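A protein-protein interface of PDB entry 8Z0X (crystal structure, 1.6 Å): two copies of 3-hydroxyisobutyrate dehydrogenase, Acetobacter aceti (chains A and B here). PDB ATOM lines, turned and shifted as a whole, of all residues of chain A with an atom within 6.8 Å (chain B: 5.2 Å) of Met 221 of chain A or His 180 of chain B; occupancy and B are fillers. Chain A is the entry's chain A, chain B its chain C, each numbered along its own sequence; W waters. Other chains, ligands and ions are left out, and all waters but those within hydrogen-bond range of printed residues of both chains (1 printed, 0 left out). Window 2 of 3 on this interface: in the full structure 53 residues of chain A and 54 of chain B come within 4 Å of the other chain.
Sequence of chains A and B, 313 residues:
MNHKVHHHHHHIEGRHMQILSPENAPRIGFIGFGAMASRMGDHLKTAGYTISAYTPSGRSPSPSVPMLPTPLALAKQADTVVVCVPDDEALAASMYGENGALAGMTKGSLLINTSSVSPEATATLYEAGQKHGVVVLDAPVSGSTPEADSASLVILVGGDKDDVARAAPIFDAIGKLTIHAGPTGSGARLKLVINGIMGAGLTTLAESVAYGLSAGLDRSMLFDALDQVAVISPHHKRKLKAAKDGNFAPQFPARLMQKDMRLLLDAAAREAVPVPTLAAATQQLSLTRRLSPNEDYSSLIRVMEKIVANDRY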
ATOM      1  N   LEU A 217      12.075 -36.482  -1.511  1.00  0.00           N
ATOM      2  CA  LEU A 217      11.390 -35.283  -1.041  1.00  0.00           C
ATOM      3  C   LEU A 217       9.943 -35.269  -1.513  1.00  0.00           C
ATOM      4  O   LEU A 217       9.648 -35.588  -2.674  1.00  0.00           O
ATOM      5  CB  LEU A 217      12.104 -34.031  -1.546  1.00  0.00           C
ATOM      6  CG  LEU A 217      13.521 -33.858  -0.998  1.00  0.00           C
ATOM      7  CD1 LEU A 217      14.097 -32.576  -1.550  1.00  0.00           C
ATOM      8  CD2 LEU A 217      13.524 -33.831   0.529  1.00  0.00           C
ATOM      9  N   ASP A 218       9.049 -34.897  -0.594  1.00  0.00           N
ATOM     10  CA  ASP A 218       7.629 -34.736  -0.898  1.00  0.00           C
ATOM     11  C   ASP A 218       7.435 -33.746  -2.041  1.00  0.00           C
ATOM     12  O   ASP A 218       8.003 -32.647  -2.045  1.00  0.00           O
ATOM     13  CB  ASP A 218       6.905 -34.268   0.377  1.00  0.00           C
ATOM     14  CG  ASP A 218       5.403 -34.081   0.187  1.00  0.00           C
ATOM     15  OD1 ASP A 218       4.976 -33.041  -0.373  1.00  0.00           O
ATOM     16  OD2 ASP A 218       4.646 -34.953   0.664  1.00  0.00           O
ATOM     17  N   ARG A 219       6.612 -34.131  -3.028  1.00  0.00           N
ATOM     18  CA  ARG A 219       6.477 -33.306  -4.224  1.00  0.00           C
ATOM     19  C   ARG A 219       5.892 -31.935  -3.902  1.00  0.00           C
ATOM     20  O   ARG A 219       6.364 -30.906  -4.404  1.00  0.00           O
ATOM     21  CB  ARG A 219       5.598 -34.009  -5.255  1.00  0.00           C
ATOM     22  CG  ARG A 219       5.455 -33.191  -6.545  1.00  0.00           C
ATOM     23  CD  ARG A 219       4.359 -33.726  -7.447  1.00  0.00           C
ATOM     24  NE  ARG A 219       4.398 -33.126  -8.778  1.00  0.00           N
ATOM     25  CZ  ARG A 219       3.571 -32.191  -9.231  1.00  0.00           C
ATOM     26  NH1 ARG A 219       2.602 -31.685  -8.480  1.00  0.00           N
ATOM     27  NH2 ARG A 219       3.684 -31.784 -10.491  1.00  0.00           N
ATOM     28  N   SER A 220       4.823 -31.898  -3.103  1.00  0.00           N
ATOM     29  CA  SER A 220       4.196 -30.612  -2.812  1.00  0.00           C
ATOM     30  C   SER A 220       5.110 -29.724  -1.976  1.00  0.00           C
ATOM     31  O   SER A 220       5.208 -28.515  -2.232  1.00  0.00           O
ATOM     32  CB  SER A 220       2.861 -30.839  -2.101  1.00  0.00           C
ATOM     33  OG  SER A 220       2.027 -31.651  -2.903  1.00  0.00           O
ATOM     34  N   MET A 221       5.761 -30.304  -0.967  1.00  0.00           N
ATOM     35  CA  MET A 221       6.773 -29.592  -0.191  1.00  0.00           C
ATOM     36  C   MET A 221       7.800 -28.947  -1.106  1.00  0.00           C
ATOM     37  O   MET A 221       8.090 -27.749  -0.995  1.00  0.00           O
ATOM     38  CB  MET A 221       7.449 -30.575   0.763  1.00  0.00           C
ATOM     39  CG  MET A 221       8.466 -29.998   1.771  1.00  0.00           C
ATOM     40  SD  MET A 221      10.048 -29.440   1.057  1.00  0.00           S
ATOM     41  CE  MET A 221      10.719 -31.006   0.503  1.00  0.00           C
ATOM     42  N   LEU A 222       8.345 -29.741  -2.029  1.00  0.00           N
ATOM     43  CA  LEU A 222       9.491 -29.308  -2.825  1.00  0.00           C
ATOM     44  C   LEU A 222       9.116 -28.182  -3.778  1.00  0.00           C
ATOM     45  O   LEU A 222       9.838 -27.189  -3.885  1.00  0.00           O
ATOM     46  CB  LEU A 222      10.045 -30.511  -3.590  1.00  0.00           C
ATOM     47  CG  LEU A 222      11.159 -30.244  -4.610  1.00  0.00           C
ATOM     48  CD1 LEU A 222      12.350 -29.582  -3.929  1.00  0.00           C
ATOM     49  CD2 LEU A 222      11.544 -31.560  -5.265  1.00  0.00           C
ATOM     50  N   PHE A 223       7.998 -28.319  -4.498  1.00  0.00           N
ATOM     51  CA  PHE A 223       7.579 -27.237  -5.376  1.00  0.00           C
ATOM     52  C   PHE A 223       7.328 -25.964  -4.582  1.00  0.00           C
ATOM     53  O   PHE A 223       7.701 -24.867  -5.018  1.00  0.00           O
ATOM     54  CB  PHE A 223       6.319 -27.617  -6.149  1.00  0.00           C
ATOM     55  CG  PHE A 223       6.578 -28.443  -7.382  1.00  0.00           C
ATOM     56  CD1 PHE A 223       7.049 -29.748  -7.283  1.00  0.00           C
ATOM     57  CD2 PHE A 223       6.310 -27.913  -8.640  1.00  0.00           C
ATOM     58  CE1 PHE A 223       7.256 -30.510  -8.423  1.00  0.00           C
ATOM     59  CE2 PHE A 223       6.522 -28.667  -9.789  1.00  0.00           C
ATOM     60  CZ  PHE A 223       6.972 -29.968  -9.677  1.00  0.00           C
ATOM     61  N   ASP A 224       6.735 -26.089  -3.391  1.00  0.00           N
ATOM     62  CA  ASP A 224       6.438 -24.877  -2.644  1.00  0.00           C
ATOM     63  C   ASP A 224       7.706 -24.249  -2.065  1.00  0.00           C
ATOM     64  O   ASP A 224       7.805 -23.015  -1.980  1.00  0.00           O
ATOM     65  CB  ASP A 224       5.475 -25.172  -1.509  1.00  0.00           C
ATOM     66  CG  ASP A 224       4.082 -25.415  -1.993  1.00  0.00           C
ATOM     67  OD1 ASP A 224       3.762 -25.104  -3.166  1.00  0.00           O
ATOM     68  OD2 ASP A 224       3.263 -25.777  -1.122  1.00  0.00           O
ATOM     69  N   ALA A 225       8.673 -25.078  -1.665  1.00  0.00           N
ATOM     70  CA  ALA A 225       9.913 -24.573  -1.077  1.00  0.00           C
ATOM     71  C   ALA A 225      10.701 -23.778  -2.098  1.00  0.00           C
ATOM     72  O   ALA A 225      11.296 -22.739  -1.782  1.00  0.00           O
ATOM     73  CB  ALA A 225      10.758 -25.733  -0.566  1.00  0.00           C
ATOM     74  N   LEU A 226      10.724 -24.265  -3.330  1.00  0.00           N
ATOM     75  CA  LEU A 226      11.523 -23.594  -4.337  1.00  0.00           C
ATOM     76  C   LEU A 226      10.934 -22.244  -4.709  1.00  0.00           C
ATOM     77  O   LEU A 226      11.661 -21.356  -5.137  1.00  0.00           O
ATOM     78  CB  LEU A 226      11.682 -24.504  -5.558  1.00  0.00           C
ATOM     79  CG  LEU A 226      12.540 -25.748  -5.299  1.00  0.00           C
ATOM     80  CD1 LEU A 226      12.611 -26.604  -6.565  1.00  0.00           C
ATOM     81  CD2 LEU A 226      13.941 -25.351  -4.851  1.00  0.00           C
ATOM     82  N   LYS A 244       3.388 -27.522 -11.016  1.00  0.00           N
ATOM     83  CA  LYS A 244       2.796 -28.201  -9.865  1.00  0.00           C
ATOM     84  C   LYS A 244       1.382 -28.644 -10.197  1.00  0.00           C
ATOM     85  O   LYS A 244       0.943 -29.727  -9.782  1.00  0.00           O
ATOM     86  CB  LYS A 244       2.782 -27.279  -8.651  1.00  0.00           C
ATOM     87  CG  LYS A 244       2.435 -28.001  -7.346  1.00  0.00           C
ATOM     88  CD  LYS A 244       2.324 -27.024  -6.191  1.00  0.00           C
ATOM     89  CE  LYS A 244       1.952 -27.761  -4.888  1.00  0.00           C
ATOM     90  NZ  LYS A 244       1.576 -26.795  -3.800  1.00  0.00           N
ATOM     91  N   VAL B 157      15.460 -27.811   6.769  1.00  0.00           N
ATOM     92  CA  VAL B 157      15.733 -28.693   7.896  1.00  0.00           C
ATOM     93  C   VAL B 157      15.018 -30.035   7.765  1.00  0.00           C
ATOM     94  O   VAL B 157      13.839 -30.107   7.396  1.00  0.00           O
ATOM     95  CB  VAL B 157      15.390 -28.016   9.244  1.00  0.00           C
ATOM     96  CG1 VAL B 157      13.914 -27.670   9.355  1.00  0.00           C
ATOM     97  CG2 VAL B 157      15.892 -28.900  10.404  1.00  0.00           C
ATOM     98  N   GLY B 158      15.756 -31.096   8.076  1.00  0.00           N
ATOM     99  CA  GLY B 158      15.226 -32.451   8.140  1.00  0.00           C
ATOM    100  C   GLY B 158      15.210 -32.941   9.580  1.00  0.00           C
ATOM    101  O   GLY B 158      16.173 -32.730  10.326  1.00  0.00           O
ATOM    102  N   GLY B 159      14.120 -33.576   9.963  1.00  0.00           N
ATOM    103  CA  GLY B 159      14.002 -34.119  11.303  1.00  0.00           C
ATOM    104  C   GLY B 159      12.545 -34.237  11.702  1.00  0.00           C
ATOM    105  O   GLY B 159      11.636 -33.911  10.948  1.00  0.00           O
ATOM    106  N   ASP B 160      12.338 -34.727  12.918  1.00  0.00           N
ATOM    107  CA  ASP B 160      10.979 -34.799  13.437  1.00  0.00           C
ATOM    108  C   ASP B 160      10.465 -33.401  13.755  1.00  0.00           C
ATOM    109  O   ASP B 160      11.216 -32.537  14.212  1.00  0.00           O
ATOM    110  CB  ASP B 160      10.937 -35.688  14.682  1.00  0.00           C
ATOM    111  CG  ASP B 160       9.564 -35.717  15.339  1.00  0.00           C
ATOM    112  OD1 ASP B 160       9.132 -34.685  15.897  1.00  0.00           O
ATOM    113  OD2 ASP B 160       8.905 -36.773  15.278  1.00  0.00           O
ATOM    114  N   LYS B 161       9.163 -33.188  13.536  1.00  0.00           N
ATOM    115  CA  LYS B 161       8.586 -31.861  13.740  1.00  0.00           C
ATOM    116  C   LYS B 161       8.800 -31.359  15.165  1.00  0.00           C
ATOM    117  O   LYS B 161       8.949 -30.152  15.377  1.00  0.00           O
ATOM    118  CB  LYS B 161       7.092 -31.874  13.395  1.00  0.00           C
ATOM    119  CG  LYS B 161       6.187 -32.504  14.444  1.00  0.00           C
ATOM    120  CD  LYS B 161       4.706 -32.131  14.246  1.00  0.00           C
ATOM    121  CE  LYS B 161       4.526 -30.704  13.732  1.00  0.00           C
ATOM    122  NZ  LYS B 161       3.087 -30.300  13.691  1.00  0.00           N
ATOM    123  N   VAL B 164      12.370 -30.022  15.341  1.00  0.00           N
ATOM    124  CA  VAL B 164      12.431 -28.749  14.629  1.00  0.00           C
ATOM    125  C   VAL B 164      11.855 -27.631  15.491  1.00  0.00           C
ATOM    126  O   VAL B 164      12.405 -26.524  15.552  1.00  0.00           O
ATOM    127  CB  VAL B 164      11.702 -28.865  13.278  1.00  0.00           C
ATOM    128  CG1 VAL B 164      11.680 -27.521  12.571  1.00  0.00           C
ATOM    129  CG2 VAL B 164      12.380 -29.904  12.413  1.00  0.00           C
ATOM    130  N   THR B 178      11.969 -20.855   7.987  1.00  0.00           N
ATOM    131  CA  THR B 178      12.376 -22.235   8.222  1.00  0.00           C
ATOM    132  C   THR B 178      11.482 -23.140   7.389  1.00  0.00           C
ATOM    133  O   THR B 178      10.265 -23.182   7.607  1.00  0.00           O
ATOM    134  CB  THR B 178      12.276 -22.585   9.709  1.00  0.00           C
ATOM    135  OG1 THR B 178      13.179 -21.751  10.443  1.00  0.00           O
ATOM    136  CG2 THR B 178      12.618 -24.051   9.958  1.00  0.00           C
ATOM    137  N   ILE B 179      12.077 -23.854   6.434  1.00  0.00           N
ATOM    138  CA  ILE B 179      11.347 -24.832   5.636  1.00  0.00           C
ATOM    139  C   ILE B 179      11.616 -26.209   6.224  1.00  0.00           C
ATOM    140  O   ILE B 179      12.762 -26.681   6.222  1.00  0.00           O
ATOM    141  CB  ILE B 179      11.751 -24.769   4.152  1.00  0.00           C
ATOM    142  CG1 ILE B 179      11.512 -23.372   3.594  1.00  0.00           C
ATOM    143  CG2 ILE B 179      10.953 -25.783   3.349  1.00  0.00           C
ATOM    144  CD1 ILE B 179      12.017 -23.184   2.168  1.00  0.00           C
ATOM    145  N   HIS B 180      10.570 -26.848   6.755  1.00  0.00           N
ATOM    146  CA  HIS B 180      10.677 -28.222   7.230  1.00  0.00           C
ATOM    147  C   HIS B 180      10.547 -29.145   6.024  1.00  0.00           C
ATOM    148  O   HIS B 180       9.456 -29.314   5.474  1.00  0.00           O
ATOM    149  CB  HIS B 180       9.612 -28.523   8.284  1.00  0.00           C
ATOM    150  CG  HIS B 180       9.756 -29.873   8.914  1.00  0.00           C
ATOM    151  ND1 HIS B 180       8.733 -30.482   9.612  1.00  0.00           N
ATOM    152  CD2 HIS B 180      10.801 -30.737   8.951  1.00  0.00           C
ATOM    153  CE1 HIS B 180       9.143 -31.659  10.054  1.00  0.00           C
ATOM    154  NE2 HIS B 180      10.390 -31.843   9.656  1.00  0.00           N
ATOM    155  N   ALA B 181      11.657 -29.732   5.598  1.00  0.00           N
ATOM    156  CA  ALA B 181      11.681 -30.431   4.320  1.00  0.00           C
ATOM    157  C   ALA B 181      11.265 -31.895   4.414  1.00  0.00           C
ATOM    158  O   ALA B 181      11.068 -32.534   3.376  1.00  0.00           O
ATOM    159  CB  ALA B 181      13.088 -30.333   3.713  1.00  0.00           C
ATOM    160  N   GLY B 182      11.097 -32.432   5.617  1.00  0.00           N
ATOM    161  CA  GLY B 182      10.798 -33.828   5.812  1.00  0.00           C
ATOM    162  C   GLY B 182      11.594 -34.395   6.972  1.00  0.00           C
ATOM    163  O   GLY B 182      12.150 -33.654   7.790  1.00  0.00           O
ATOM    164  N   PRO B 183      11.692 -35.719   7.039  1.00  0.00           N
ATOM    165  CA  PRO B 183      12.493 -36.367   8.094  1.00  0.00           C
ATOM    166  C   PRO B 183      13.992 -36.195   7.898  1.00  0.00           C
ATOM    167  O   PRO B 183      14.413 -35.532   6.942  1.00  0.00           O
ATOM    168  CB  PRO B 183      12.094 -37.844   7.979  1.00  0.00           C
ATOM    169  CG  PRO B 183      11.592 -38.001   6.596  1.00  0.00           C
ATOM    170  CD  PRO B 183      10.964 -36.692   6.208  1.00  0.00           C
ATOM    171  N   LEU B 190      17.338 -31.103   0.041  1.00  0.00           N
ATOM    172  CA  LEU B 190      16.814 -29.853  -0.498  1.00  0.00           C
ATOM    173  C   LEU B 190      17.941 -28.861  -0.764  1.00  0.00           C
ATOM    174  O   LEU B 190      17.888 -28.097  -1.735  1.00  0.00           O
ATOM    175  CB  LEU B 190      15.762 -29.279   0.466  1.00  0.00           C
ATOM    176  CG  LEU B 190      15.055 -27.994   0.053  1.00  0.00           C
ATOM    177  CD1 LEU B 190      14.412 -28.076  -1.347  1.00  0.00           C
ATOM    178  CD2 LEU B 190      14.000 -27.629   1.114  1.00  0.00           C
HETATM  179  O   HOH W   1       9.821 -34.613   2.268  1.00  0.00           O
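The backbone NH (N) of Ala 181 of chain B is in hydrogen-bond range of the backbone carbonyl oxygen (O) of Val 157 of chain B, 2.9 Å away. The backbone NH of Met 221 of chain A sits at hydrogen-bond distance from the side-chain carboxylate of Asp 218 of chain A (2.9 Å). The backbone carbonyl oxygen (O) of Ile 179 of chain B is in hydrogen-bond range of the backbone NH (N) of Val 157 of chain B (3.0 Å). The backbone carbonyl oxygen (O) of Gly 159 of chain B sits at hydrogen-bond distance from a ring nitrogen (NE2) of His 180 of chain B (2.7 Å). NE2 of His 180 of chain B is in hydrogen-bond range of O of Gly 182 of chain B (3.1 Å).
Among the printed residues, merely in contact across the chains: Leu 217 of chain A with Ala 181 of chain B (3.98 Å), Leu 217 of chain A with Leu 190 of chain B (3.9 Å), Met 221 of chain A with His 180 of chain B (3.9 Å), Met 221 of chain A with Ala 181 of chain B (3.3 Å), Leu 222 of chain A with Leu 190 of chain B (3.6 Å) and Ala 225 of chain A with Ile 179 of chain B (3.9 Å).
Of the 13 printed residues of chain B, 4 touch a printed residue of chain A. Along chain B the printed residues that touch a printed residue of chain A span positions 179 to 190. Hydrophobic or aromatic side chains of chain A that line the printed part of chain B: Leu 217, Met 221, Leu 222 and Ala 225. Among the printed residues, 6 pairs touch across the chains.
Met 221 of chain A touches two residues of chain B. Printed residues of chain A within 4 Å of His 180 of chain B: Met 221 (3.9 Å). Of the printed residues of chain A, Ala 181 of chain B touches Leu 217 (3.98 Å) and Met 221 (3.3 Å). Of the printed residues of chain A, Leu 190 of chain B touches Leu 217 and Leu 222. Lys 161 of chain B touches none of the printed residues of chain A. The nearest residue of chain B that does not touch Met 221 of chain A is Leu 190 of chain B (4.3 Å). The nearest printed residue of chain A that does not touch His 180 of chain B is Ala 225 of chain A (7.1 Å). The nearest printed residue of chain A that does not touch Ile 179 of chain B is Met 221 of chain A (4.4 Å).
Water W1 bridges O of Ala 181 of chain B (2.7 Å) and N of Asp 218 of chain A (3.0 Å).
No position is printed for both chains.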
